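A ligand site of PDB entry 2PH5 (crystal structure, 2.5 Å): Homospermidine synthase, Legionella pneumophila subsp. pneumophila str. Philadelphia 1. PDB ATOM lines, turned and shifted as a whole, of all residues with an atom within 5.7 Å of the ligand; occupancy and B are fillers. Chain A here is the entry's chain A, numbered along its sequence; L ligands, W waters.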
ATOM      1  N   LEU A  19      16.987 -28.243  24.901  1.00  0.00           N
ATOM      2  CA  LEU A  19      17.029 -26.954  24.224  1.00  0.00           C
ATOM      3  C   LEU A  19      15.613 -26.641  23.807  1.00  0.00           C
ATOM      4  O   LEU A  19      14.922 -27.455  23.204  1.00  0.00           O
ATOM      5  CB  LEU A  19      17.964 -26.954  23.018  1.00  0.00           C
ATOM      6  CG  LEU A  19      17.444 -27.537  21.714  1.00  0.00           C
ATOM      7  CD1 LEU A  19      18.336 -27.102  20.559  1.00  0.00           C
ATOM      8  CD2 LEU A  19      17.374 -29.038  21.832  1.00  0.00           C
ATOM      9  N   GLY A  20      15.196 -25.423  24.131  1.00  0.00           N
ATOM     10  CA  GLY A  20      13.841 -24.989  23.843  1.00  0.00           C
ATOM     11  C   GLY A  20      13.092 -25.109  25.148  1.00  0.00           C
ATOM     12  O   GLY A  20      13.369 -26.027  25.925  1.00  0.00           O
ATOM     13  N   PHE A  21      12.171 -24.198  25.419  1.00  0.00           N
ATOM     14  CA  PHE A  21      11.400 -24.269  26.652  1.00  0.00           C
ATOM     15  C   PHE A  21      10.006 -23.681  26.444  1.00  0.00           C
ATOM     16  O   PHE A  21       9.557 -22.815  27.199  1.00  0.00           O
ATOM     17  CB  PHE A  21      12.109 -23.523  27.791  1.00  0.00           C
ATOM     18  CG  PHE A  21      11.782 -24.048  29.174  1.00  0.00           C
ATOM     19  CD1 PHE A  21      11.956 -25.398  29.478  1.00  0.00           C
ATOM     20  CD2 PHE A  21      11.338 -23.181  30.174  1.00  0.00           C
ATOM     21  CE1 PHE A  21      11.679 -25.876  30.770  1.00  0.00           C
ATOM     22  CE2 PHE A  21      11.068 -23.652  31.464  1.00  0.00           C
ATOM     23  CZ  PHE A  21      11.241 -25.002  31.768  1.00  0.00           C
ATOM     24  N   GLY A  22       9.328 -24.181  25.408  1.00  0.00           N
ATOM     25  CA  GLY A  22       7.993 -23.698  25.110  1.00  0.00           C
ATOM     26  C   GLY A  22       6.884 -24.557  25.707  1.00  0.00           C
ATOM     27  O   GLY A  22       6.968 -24.994  26.861  1.00  0.00           O
ATOM     28  N   CYS A  23       5.861 -24.797  24.899  1.00  0.00           N
ATOM     29  CA  CYS A  23       4.696 -25.598  25.289  1.00  0.00           C
ATOM     30  C   CYS A  23       5.110 -26.983  25.756  1.00  0.00           C
ATOM     31  O   CYS A  23       4.755 -27.407  26.863  1.00  0.00           O
ATOM     32  CB  CYS A  23       3.744 -25.717  24.089  1.00  0.00           C
ATOM     33  SG  CYS A  23       3.466 -24.154  23.188  1.00  0.00           S
ATOM     34  N   VAL A  24       5.862 -27.696  24.922  1.00  0.00           N
ATOM     35  CA  VAL A  24       6.332 -29.040  25.237  1.00  0.00           C
ATOM     36  C   VAL A  24       7.379 -29.072  26.368  1.00  0.00           C
ATOM     37  O   VAL A  24       7.206 -29.768  27.369  1.00  0.00           O
ATOM     38  CB  VAL A  24       6.931 -29.728  23.977  1.00  0.00           C
ATOM     39  CG1 VAL A  24       7.452 -31.116  24.323  1.00  0.00           C
ATOM     40  CG2 VAL A  24       5.872 -29.818  22.892  1.00  0.00           C
ATOM     41  N   GLY A  25       8.458 -28.328  26.193  1.00  0.00           N
ATOM     42  CA  GLY A  25       9.526 -28.295  27.177  1.00  0.00           C
ATOM     43  C   GLY A  25       9.088 -28.047  28.602  1.00  0.00           C
ATOM     44  O   GLY A  25       9.538 -28.755  29.510  1.00  0.00           O
ATOM     45  N   ILE A  46      18.356 -24.451  27.474  1.00  0.00           N
ATOM     46  CA  ILE A  46      18.827 -23.402  26.586  1.00  0.00           C
ATOM     47  C   ILE A  46      17.668 -23.027  25.689  1.00  0.00           C
ATOM     48  O   ILE A  46      17.098 -23.902  25.028  1.00  0.00           O
ATOM     49  CB  ILE A  46      19.965 -23.897  25.699  1.00  0.00           C
ATOM     50  CG1 ILE A  46      21.030 -24.566  26.575  1.00  0.00           C
ATOM     51  CG2 ILE A  46      20.519 -22.747  24.872  1.00  0.00           C
ATOM     52  CD1 ILE A  46      22.230 -25.057  25.810  1.00  0.00           C
ATOM     53  N   ALA A  47      17.302 -21.744  25.663  1.00  0.00           N
ATOM     54  CA  ALA A  47      16.183 -21.265  24.847  1.00  0.00           C
ATOM     55  C   ALA A  47      16.441 -19.833  24.387  1.00  0.00           C
ATOM     56  O   ALA A  47      17.167 -19.089  25.036  1.00  0.00           O
ATOM     57  CB  ALA A  47      14.892 -21.351  25.628  1.00  0.00           C
ATOM     58  N   ALA A  48      15.827 -19.431  23.276  1.00  0.00           N
ATOM     59  CA  ALA A  48      16.029 -18.085  22.752  1.00  0.00           C
ATOM     60  C   ALA A  48      15.167 -17.014  23.408  1.00  0.00           C
ATOM     61  O   ALA A  48      15.595 -15.873  23.552  1.00  0.00           O
ATOM     62  CB  ALA A  48      15.792 -18.076  21.256  1.00  0.00           C
ATOM     63  N   GLU A  49      13.961 -17.389  23.801  1.00  0.00           N
ATOM     64  CA  GLU A  49      13.044 -16.453  24.435  1.00  0.00           C
ATOM     65  C   GLU A  49      12.765 -16.888  25.861  1.00  0.00           C
ATOM     66  O   GLU A  49      12.612 -18.091  26.131  1.00  0.00           O
ATOM     67  CB  GLU A  49      11.719 -16.384  23.672  1.00  0.00           C
ATOM     68  CG  GLU A  49      11.813 -15.876  22.259  1.00  0.00           C
ATOM     69  CD  GLU A  49      11.076 -16.764  21.272  1.00  0.00           C
ATOM     70  OE1 GLU A  49      11.597 -17.856  20.954  1.00  0.00           O
ATOM     71  OE2 GLU A  49       9.963 -16.372  20.832  1.00  0.00           O
ATOM     72  N   GLN A  66      19.739 -18.002  25.162  1.00  0.00           N
ATOM     73  CA  GLN A  66      20.607 -17.869  24.009  1.00  0.00           C
ATOM     74  C   GLN A  66      19.980 -18.383  22.730  1.00  0.00           C
ATOM     75  O   GLN A  66      19.245 -19.359  22.743  1.00  0.00           O
ATOM     76  CB  GLN A  66      21.939 -18.592  24.234  1.00  0.00           C
ATOM     77  CG  GLN A  66      22.858 -18.506  23.030  1.00  0.00           C
ATOM     78  CD  GLN A  66      24.308 -18.192  23.398  1.00  0.00           C
ATOM     79  OE1 GLN A  66      24.958 -18.949  24.124  1.00  0.00           O
ATOM     80  NE2 GLN A  66      24.811 -17.070  22.893  1.00  0.00           N
ATOM     81  N   GLN A  67      20.282 -17.705  21.632  1.00  0.00           N
ATOM     82  CA  GLN A  67      19.766 -18.107  20.331  1.00  0.00           C
ATOM     83  C   GLN A  67      20.782 -19.047  19.669  1.00  0.00           C
ATOM     84  O   GLN A  67      21.951 -18.698  19.536  1.00  0.00           O
ATOM     85  CB  GLN A  67      19.541 -16.862  19.456  1.00  0.00           C
ATOM     86  CG  GLN A  67      19.174 -17.168  18.015  1.00  0.00           C
ATOM     87  CD  GLN A  67      18.976 -15.897  17.196  1.00  0.00           C
ATOM     88  OE1 GLN A  67      18.106 -15.071  17.505  1.00  0.00           O
ATOM     89  NE2 GLN A  67      19.787 -15.725  16.167  1.00  0.00           N
ATOM     90  N   ILE A  68      20.335 -20.231  19.289  1.00  0.00           N
ATOM     91  CA  ILE A  68      21.217 -21.216  18.665  1.00  0.00           C
ATOM     92  C   ILE A  68      21.231 -21.003  17.160  1.00  0.00           C
ATOM     93  O   ILE A  68      20.189 -21.023  16.510  1.00  0.00           O
ATOM     94  CB  ILE A  68      20.763 -22.666  18.984  1.00  0.00           C
ATOM     95  CG1 ILE A  68      20.813 -22.897  20.503  1.00  0.00           C
ATOM     96  CG2 ILE A  68      21.639 -23.664  18.261  1.00  0.00           C
ATOM     97  CD1 ILE A  68      22.176 -22.589  21.127  1.00  0.00           C
ATOM     98  N   THR A  69      22.413 -20.822  16.603  1.00  0.00           N
ATOM     99  CA  THR A  69      22.518 -20.570  15.172  1.00  0.00           C
ATOM    100  C   THR A  69      23.464 -21.577  14.544  1.00  0.00           C
ATOM    101  O   THR A  69      24.101 -22.372  15.227  1.00  0.00           O
ATOM    102  CB  THR A  69      23.079 -19.182  14.929  1.00  0.00           C
ATOM    103  OG1 THR A  69      24.404 -19.124  15.471  1.00  0.00           O
ATOM    104  CG2 THR A  69      22.210 -18.130  15.600  1.00  0.00           C
ATOM    105  N   VAL A  90      13.356 -29.998  21.993  1.00  0.00           N
ATOM    106  CA  VAL A  90      11.964 -29.561  21.959  1.00  0.00           C
ATOM    107  C   VAL A  90      11.931 -28.095  21.510  1.00  0.00           C
ATOM    108  O   VAL A  90      11.151 -27.287  22.039  1.00  0.00           O
ATOM    109  CB  VAL A  90      11.299 -29.720  23.355  1.00  0.00           C
ATOM    110  CG1 VAL A  90      11.205 -31.190  23.722  1.00  0.00           C
ATOM    111  CG2 VAL A  90      12.079 -28.964  24.400  1.00  0.00           C
ATOM    112  N   SER A  91      12.788 -27.773  20.542  1.00  0.00           N
ATOM    113  CA  SER A  91      12.906 -26.421  19.985  1.00  0.00           C
ATOM    114  C   SER A  91      12.249 -26.309  18.627  1.00  0.00           C
ATOM    115  O   SER A  91      11.601 -27.240  18.151  1.00  0.00           O
ATOM    116  CB  SER A  91      14.379 -26.036  19.828  1.00  0.00           C
ATOM    117  OG  SER A  91      15.021 -26.891  18.878  1.00  0.00           O
ATOM    118  N   ILE A  92      12.419 -25.150  18.009  1.00  0.00           N
ATOM    119  CA  ILE A  92      11.909 -24.907  16.677  1.00  0.00           C
ATOM    120  C   ILE A  92      12.984 -24.119  15.920  1.00  0.00           C
ATOM    121  O   ILE A  92      13.847 -23.474  16.530  1.00  0.00           O
ATOM    122  CB  ILE A  92      10.567 -24.135  16.727  1.00  0.00           C
ATOM    123  CG1 ILE A  92       9.733 -24.541  15.526  1.00  0.00           C
ATOM    124  CG2 ILE A  92      10.799 -22.620  16.771  1.00  0.00           C
ATOM    125  CD1 ILE A  92       9.223 -25.963  15.634  1.00  0.00           C
ATOM    126  N   GLY A  93      12.966 -24.209  14.590  1.00  0.00           N
ATOM    127  CA  GLY A  93      13.965 -23.476  13.814  1.00  0.00           C
ATOM    128  C   GLY A  93      15.413 -23.923  13.932  1.00  0.00           C
ATOM    129  O   GLY A  93      16.304 -23.223  13.457  1.00  0.00           O
ATOM    130  N   ILE A  94      15.673 -25.065  14.571  1.00  0.00           N
ATOM    131  CA  ILE A  94      17.052 -25.558  14.677  1.00  0.00           C
ATOM    132  C   ILE A  94      17.169 -26.909  13.980  1.00  0.00           C
ATOM    133  O   ILE A  94      16.382 -27.815  14.222  1.00  0.00           O
ATOM    134  CB  ILE A  94      17.511 -25.724  16.137  1.00  0.00           C
ATOM    135  CG1 ILE A  94      17.359 -24.413  16.893  1.00  0.00           C
ATOM    136  CG2 ILE A  94      18.974 -26.146  16.168  1.00  0.00           C
ATOM    137  CD1 ILE A  94      17.747 -24.506  18.357  1.00  0.00           C
ATOM    138  N   ALA A 113      10.427 -34.273  19.076  1.00  0.00           N
ATOM    139  CA  ALA A 113       9.018 -34.531  18.830  1.00  0.00           C
ATOM    140  C   ALA A 113       8.690 -34.166  17.381  1.00  0.00           C
ATOM    141  O   ALA A 113       7.557 -34.296  16.937  1.00  0.00           O
ATOM    142  CB  ALA A 113       8.179 -33.718  19.806  1.00  0.00           C
ATOM    143  N   ALA A 114       9.693 -33.703  16.630  1.00  0.00           N
ATOM    144  CA  ALA A 114       9.513 -33.350  15.217  1.00  0.00           C
ATOM    145  C   ALA A 114      10.813 -32.925  14.538  1.00  0.00           C
ATOM    146  O   ALA A 114      11.654 -32.246  15.141  1.00  0.00           O
ATOM    147  CB  ALA A 114       8.458 -32.245  15.078  1.00  0.00           C
ATOM    148  N   GLU A 116      13.072 -30.721  12.354  1.00  0.00           N
ATOM    149  CA  GLU A 116      13.068 -29.315  11.958  1.00  0.00           C
ATOM    150  C   GLU A 116      14.388 -28.895  11.291  1.00  0.00           C
ATOM    151  O   GLU A 116      15.442 -29.460  11.563  1.00  0.00           O
ATOM    152  CB  GLU A 116      12.827 -28.435  13.182  1.00  0.00           C
ATOM    153  CG  GLU A 116      11.481 -28.617  13.850  1.00  0.00           C
ATOM    154  CD  GLU A 116      10.398 -27.784  13.206  1.00  0.00           C
ATOM    155  OE1 GLU A 116      10.636 -26.565  13.005  1.00  0.00           O
ATOM    156  OE2 GLU A 116       9.305 -28.325  12.899  1.00  0.00           O
ATOM    157  N   THR A 155      10.762 -37.683  15.837  1.00  0.00           N
ATOM    158  CA  THR A 155       9.317 -37.501  15.764  1.00  0.00           C
ATOM    159  C   THR A 155       8.575 -38.409  16.723  1.00  0.00           C
ATOM    160  O   THR A 155       7.647 -39.117  16.330  1.00  0.00           O
ATOM    161  CB  THR A 155       8.787 -37.784  14.337  1.00  0.00           C
ATOM    162  OG1 THR A 155       9.184 -39.099  13.931  1.00  0.00           O
ATOM    163  CG2 THR A 155       9.365 -36.763  13.343  1.00  0.00           C
ATOM    164  N   HIS A 156       8.990 -38.385  17.989  1.00  0.00           N
ATOM    165  CA  HIS A 156       8.352 -39.232  18.987  1.00  0.00           C
ATOM    166  C   HIS A 156       7.541 -38.440  19.998  1.00  0.00           C
ATOM    167  O   HIS A 156       7.907 -38.343  21.167  1.00  0.00           O
ATOM    168  CB  HIS A 156       9.392 -40.078  19.715  1.00  0.00           C
ATOM    169  CG  HIS A 156       8.802 -41.177  20.541  1.00  0.00           C
ATOM    170  ND1 HIS A 156       8.570 -42.440  20.046  1.00  0.00           N
ATOM    171  CD2 HIS A 156       8.334 -41.171  21.812  1.00  0.00           C
ATOM    172  CE1 HIS A 156       7.973 -43.170  20.979  1.00  0.00           C
ATOM    173  NE2 HIS A 156       7.821 -42.422  22.048  1.00  0.00           N
ATOM    174  N   GLY A 157       6.433 -37.855  19.549  1.00  0.00           N
ATOM    175  CA  GLY A 157       5.567 -37.104  20.435  1.00  0.00           C
ATOM    176  C   GLY A 157       4.255 -37.873  20.470  1.00  0.00           C
ATOM    177  O   GLY A 157       4.261 -39.082  20.284  1.00  0.00           O
ATOM    178  N   ALA A 158       3.140 -37.187  20.715  1.00  0.00           N
ATOM    179  CA  ALA A 158       1.849 -37.863  20.741  1.00  0.00           C
ATOM    180  C   ALA A 158       1.568 -38.257  19.288  1.00  0.00           C
ATOM    181  O   ALA A 158       1.276 -39.408  18.984  1.00  0.00           O
ATOM    182  CB  ALA A 158       0.770 -36.927  21.281  1.00  0.00           C
ATOM    183  N   ASN A 159       1.651 -37.296  18.383  1.00  0.00           N
ATOM    184  CA  ASN A 159       1.482 -37.593  16.972  1.00  0.00           C
ATOM    185  C   ASN A 159       2.164 -36.529  16.144  1.00  0.00           C
ATOM    186  O   ASN A 159       1.793 -35.354  16.192  1.00  0.00           O
ATOM    187  CB  ASN A 159       0.002 -37.745  16.550  1.00  0.00           C
ATOM    188  CG  ASN A 159      -0.775 -36.465  16.674  1.00  0.00           C
ATOM    189  OD1 ASN A 159      -1.799 -36.292  16.014  1.00  0.00           O
ATOM    190  ND2 ASN A 159      -0.306 -35.567  17.523  1.00  0.00           N
ATOM    191  N   PRO A 160       3.187 -36.925  15.389  1.00  0.00           N
ATOM    192  CA  PRO A 160       3.717 -38.289  15.260  1.00  0.00           C
ATOM    193  C   PRO A 160       4.269 -38.862  16.560  1.00  0.00           C
ATOM    194  O   PRO A 160       4.683 -38.115  17.450  1.00  0.00           O
ATOM    195  CB  PRO A 160       4.811 -38.129  14.226  1.00  0.00           C
ATOM    196  CG  PRO A 160       5.375 -36.792  14.607  1.00  0.00           C
ATOM    197  CD  PRO A 160       4.110 -35.955  14.787  1.00  0.00           C
ATOM    198  N   GLY A 161       4.281 -40.192  16.664  1.00  0.00           N
ATOM    199  CA  GLY A 161       4.813 -40.827  17.844  1.00  0.00           C
ATOM    200  C   GLY A 161       3.912 -41.875  18.452  1.00  0.00           C
ATOM    201  O   GLY A 161       3.812 -42.998  17.960  1.00  0.00           O
ATOM    202  N   TRP A 226      -2.220 -26.091  22.269  1.00  0.00           N
ATOM    203  CA  TRP A 226      -0.794 -26.279  22.006  1.00  0.00           C
ATOM    204  C   TRP A 226      -0.332 -25.136  21.118  1.00  0.00           C
ATOM    205  O   TRP A 226      -1.080 -24.178  20.911  1.00  0.00           O
ATOM    206  CB  TRP A 226      -0.494 -27.620  21.339  1.00  0.00           C
ATOM    207  CG  TRP A 226      -1.358 -27.948  20.172  1.00  0.00           C
ATOM    208  CD1 TRP A 226      -2.683 -28.276  20.207  1.00  0.00           C
ATOM    209  CD2 TRP A 226      -0.951 -28.056  18.799  1.00  0.00           C
ATOM    210  NE1 TRP A 226      -3.129 -28.583  18.939  1.00  0.00           N
ATOM    211  CE2 TRP A 226      -2.093 -28.465  18.056  1.00  0.00           C
ATOM    212  CE3 TRP A 226       0.267 -27.862  18.127  1.00  0.00           C
ATOM    213  CZ2 TRP A 226      -2.045 -28.674  16.670  1.00  0.00           C
ATOM    214  CZ3 TRP A 226       0.308 -28.078  16.743  1.00  0.00           C
ATOM    215  CH2 TRP A 226      -0.848 -28.479  16.038  1.00  0.00           C
ATOM    216  N   SER A 227       0.883 -25.221  20.596  1.00  0.00           N
ATOM    217  CA  SER A 227       1.417 -24.152  19.765  1.00  0.00           C
ATOM    218  C   SER A 227       0.476 -23.631  18.687  1.00  0.00           C
ATOM    219  O   SER A 227       0.097 -24.364  17.764  1.00  0.00           O
ATOM    220  CB  SER A 227       2.715 -24.579  19.091  1.00  0.00           C
ATOM    221  OG  SER A 227       3.165 -23.542  18.246  1.00  0.00           O
ATOM    222  N   VAL A 396       1.480 -35.499  24.994  1.00  0.00           N
ATOM    223  CA  VAL A 396       2.700 -35.371  24.213  1.00  0.00           C
ATOM    224  C   VAL A 396       3.944 -35.692  25.018  1.00  0.00           C
ATOM    225  O   VAL A 396       4.835 -36.401  24.541  1.00  0.00           O
ATOM    226  CB  VAL A 396       2.845 -33.948  23.652  1.00  0.00           C
ATOM    227  CG1 VAL A 396       3.962 -33.909  22.623  1.00  0.00           C
ATOM    228  CG2 VAL A 396       1.527 -33.486  23.042  1.00  0.00           C
HETATM  229  P1  LIG L   1       7.223 -23.391  21.166  1.00  0.00           P
HETATM  230  O1  LIG L   1       7.294 -22.424  20.015  1.00  0.00           O
HETATM  231  O2  LIG L   1       6.201 -23.149  22.219  1.00  0.00           O
HETATM  232  O3  LIG L   1       8.663 -23.523  21.892  1.00  0.00           O
HETATM  233  C1  LIG L   1       9.845 -23.710  21.126  1.00  0.00           C
HETATM  234  C2  LIG L   1      11.033 -23.176  21.946  1.00  0.00           C
HETATM  235  O4  LIG L   1      12.180 -23.338  21.133  1.00  0.00           O
HETATM  236  C3  LIG L   1      10.945 -21.693  22.310  1.00  0.00           C
HETATM  237  O5  LIG L   1      11.096 -21.518  23.725  1.00  0.00           O
HETATM  238  C4  LIG L   1      12.079 -21.048  21.553  1.00  0.00           C
HETATM  239  O6  LIG L   1      12.674 -19.937  22.165  1.00  0.00           O
HETATM  240  C5  LIG L   1      13.025 -22.225  21.287  1.00  0.00           C
HETATM  241  N1  LIG L   1      13.838 -22.121  20.068  1.00  0.00           N
HETATM  242  C6  LIG L   1      13.426 -21.476  18.897  1.00  0.00           C
HETATM  243  N2  LIG L   1      14.454 -20.852  18.287  1.00  0.00           N
HETATM  244  C7  LIG L   1      15.541 -21.067  19.058  1.00  0.00           C
HETATM  245  C8  LIG L   1      16.872 -20.667  18.916  1.00  0.00           C
HETATM  246  N3  LIG L   1      17.328 -19.942  17.891  1.00  0.00           N
HETATM  247  N4  LIG L   1      17.755 -21.060  19.916  1.00  0.00           N
HETATM  248  C9  LIG L   1      17.356 -21.814  20.999  1.00  0.00           C
HETATM  249  N5  LIG L   1      16.053 -22.226  21.154  1.00  0.00           N
HETATM  250  C10 LIG L   1      15.184 -21.842  20.176  1.00  0.00           C
HETATM  251  O7  LIG L   1       6.916 -24.799  20.497  1.00  0.00           O
HETATM  252  P2  LIG L   1       6.779 -26.280  21.090  1.00  0.00           P
HETATM  253  O8  LIG L   1       5.533 -26.861  20.535  1.00  0.00           O
HETATM  254  O9  LIG L   1       6.952 -26.213  22.580  1.00  0.00           O
HETATM  255  O10 LIG L   1       8.072 -26.804  20.334  1.00  0.00           O
HETATM  256  C11 LIG L   1       8.572 -28.121  20.358  1.00  0.00           C
HETATM  257  C12 LIG L   1       8.067 -28.757  19.076  1.00  0.00           C
HETATM  258  O11 LIG L   1       7.404 -29.955  19.401  1.00  0.00           O
HETATM  259  C13 LIG L   1       7.961 -28.550  17.581  1.00  0.00           C
HETATM  260  O12 LIG L   1       9.132 -28.965  16.903  1.00  0.00           O
HETATM  261  C14 LIG L   1       6.746 -29.402  17.246  1.00  0.00           C
HETATM  262  O13 LIG L   1       6.697 -29.791  15.907  1.00  0.00           O
HETATM  263  C15 LIG L   1       6.834 -30.544  18.242  1.00  0.00           C
HETATM  264  N6  LIG L   1       5.559 -31.118  18.727  1.00  0.00           N
HETATM  265  C16 LIG L   1       5.291 -32.455  18.533  1.00  0.00           C
HETATM  266  C17 LIG L   1       4.064 -32.961  19.025  1.00  0.00           C
HETATM  267  C18 LIG L   1       3.684 -34.393  18.870  1.00  0.00           C
HETATM  268  O14 LIG L   1       2.484 -34.790  19.401  1.00  0.00           O
HETATM  269  N7  LIG L   1       4.472 -35.277  18.286  1.00  0.00           N
HETATM  270  C19 LIG L   1       3.142 -32.109  19.706  1.00  0.00           C
HETATM  271  C20 LIG L   1       3.453 -30.748  19.875  1.00  0.00           C
HETATM  272  C21 LIG L   1       4.651 -30.252  19.405  1.00  0.00           C
HETATM  273  O   HOH W   1       3.779 -29.764  15.433  1.00  0.00           O
HETATM  274  O   HOH W   2       9.049 -26.531  23.791  1.00  0.00           O
HETATM  275  O   HOH W   3       5.780 -23.282  17.942  1.00  0.00           O
HETATM  276  O   HOH W   4       0.957 -30.726  21.766  1.00  0.00           O
HETATM  277  O   HOH W   5       9.017 -19.303  24.918  1.00  0.00           O
HETATM  278  O   HOH W   6      11.089 -20.165  25.844  1.00  0.00           O
HETATM  279  O   HOH W   7       5.994 -20.817  23.539  1.00  0.00           O
HETATM  280  O   HOH W   8       0.928 -32.332  17.054  1.00  0.00           O
HETATM  281  O   HOH W   9       2.919 -27.254  20.969  1.00  0.00           O
HETATM  282  O   HOH W  10      12.137 -30.319  16.797  1.00  0.00           O
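O6 of the ligand sits at hydrogen-bond distance from N of Glu 49 (3.3 Å).
An oxygen (O6) of the ligand sits at hydrogen-bond distance from the side-chain carboxylate of Glu 49.
The backbone NH (N) of Ile 68 sits at hydrogen-bond distance from a nitrogen (N4) of the ligand.
O of Ile 68 is in hydrogen-bond range of N3 of the ligand (3.4 Å).
An oxygen (O14) of the ligand sits at hydrogen-bond distance from the backbone NH (N) of Ala 158, at 2.8 Å.
The backbone NH (N) of Asn 159 sits at hydrogen-bond distance from an oxygen (O14) of the ligand (2.8 Å).
O of Asn 159 sits close to N7 of the ligand, 3.4 Å away.
ND2 of Asn 159 is in hydrogen-bond range of O14 of the ligand (3.5 Å).
The backbone NH of Cys 23 lies within hydrogen-bond range of an oxygen (O9) of the ligand, at 2.9 Å.
SG of Cys 23 sits at hydrogen-bond distance from O2 of the ligand.
O of Pro 160 sits at hydrogen-bond distance from N7 of the ligand (3.0 Å).
The backbone NH (N) of Val 24 is in hydrogen-bond range of an oxygen (O9) of the ligand (3.0 Å).
The backbone carbonyl oxygen (O) of Ser 91 is in hydrogen-bond range of an oxygen (O12) of the ligand (3.3 Å).
The backbone NH (N) of Phe 21 is in hydrogen-bond range of an oxygen (O5) of the ligand.
An oxygen (O6) of the ligand lies within hydrogen-bond range of the backbone NH (N) of Ala 48, at 3.4 Å.
The backbone carbonyl oxygen (O) of Ile 92 sits close to a nitrogen (N2) of the ligand (3.2 Å).
The backbone NH (N) of Gly 157 sits close to a nitrogen (N7) of the ligand (3.5 Å).
CA of Gly 20 touches O4 of the ligand, 3.6 Å away.
Gly 22 touches the ligand.
Ala 47 touches the ligand.
O of Gln 66 touches C9 of the ligand, at 3.6 Å.
Gln 67 touches the ligand (CG to N3, 3.3 Å).
Val 90 touches the ligand.
CD1 of Ile 94 touches N4 of the ligand, at 3.8 Å.
Ala 113 touches the ligand (O to C16, 3.3 Å).
Ala 114 touches the ligand.
CG of Glu 116 touches O12 of the ligand (3.9 Å).
CB of Ser 227 touches O8 of the ligand, 3.9 Å away.
CG1 of Val 396 touches C19 of the ligand, at 3.5 Å.
Hydrophobic or aromatic side chains within 4 Å of the ligand: Val 24, Ala 48, Ile 68, Ile 92, Ile 94, Ala 113, Ala 114, Ala 158, Pro 160 and Val 396.
The backbone NH (N) of Val 90 is in hydrogen-bond range of the backbone carbonyl oxygen (O) of Leu 19 (3.2 Å).
The backbone NH of Ser 91 is in hydrogen-bond range of the backbone carbonyl oxygen of Leu 19, at 3.4 Å.
The backbone NH (N) of Ala 48 sits close to the backbone carbonyl oxygen (O) of Gln 66, 3.5 Å away.
N of Gln 66 is in hydrogen-bond range of O of Ala 47, at 2.8 Å.
The backbone carbonyl oxygen of Ile 46 sits at hydrogen-bond distance from the backbone NH of Gly 20.
Water W2 lies within hydrogen-bond range of an oxygen (O9) of the ligand (2.4 Å), the backbone carbonyl oxygen of Val 90 (2.8 Å), the backbone NH of Gly 22 (2.9 Å) and the backbone NH of Gly 25 (3.1 Å).
Water W6 lies within hydrogen-bond range of an oxygen (O5) of the ligand (2.5 Å), the backbone carbonyl oxygen (O) of Glu 49 (2.6 Å) and the backbone carbonyl oxygen (O) of Phe 21 (3.3 Å).
Water W9 bridges an oxygen (O8) of the ligand and the backbone NH of Ser 227.
Water W3 lies within hydrogen-bond range of OG of Ser 227 (2.6 Å) and O1 of the ligand (2.7 Å).
Water W10 lies within hydrogen-bond range of the backbone carbonyl oxygen (O) of Ala 114 (2.6 Å), an oxygen (O12) of the ligand (3.3 Å) and the backbone carbonyl oxygen (O) of Ser 91 (3.4 Å).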
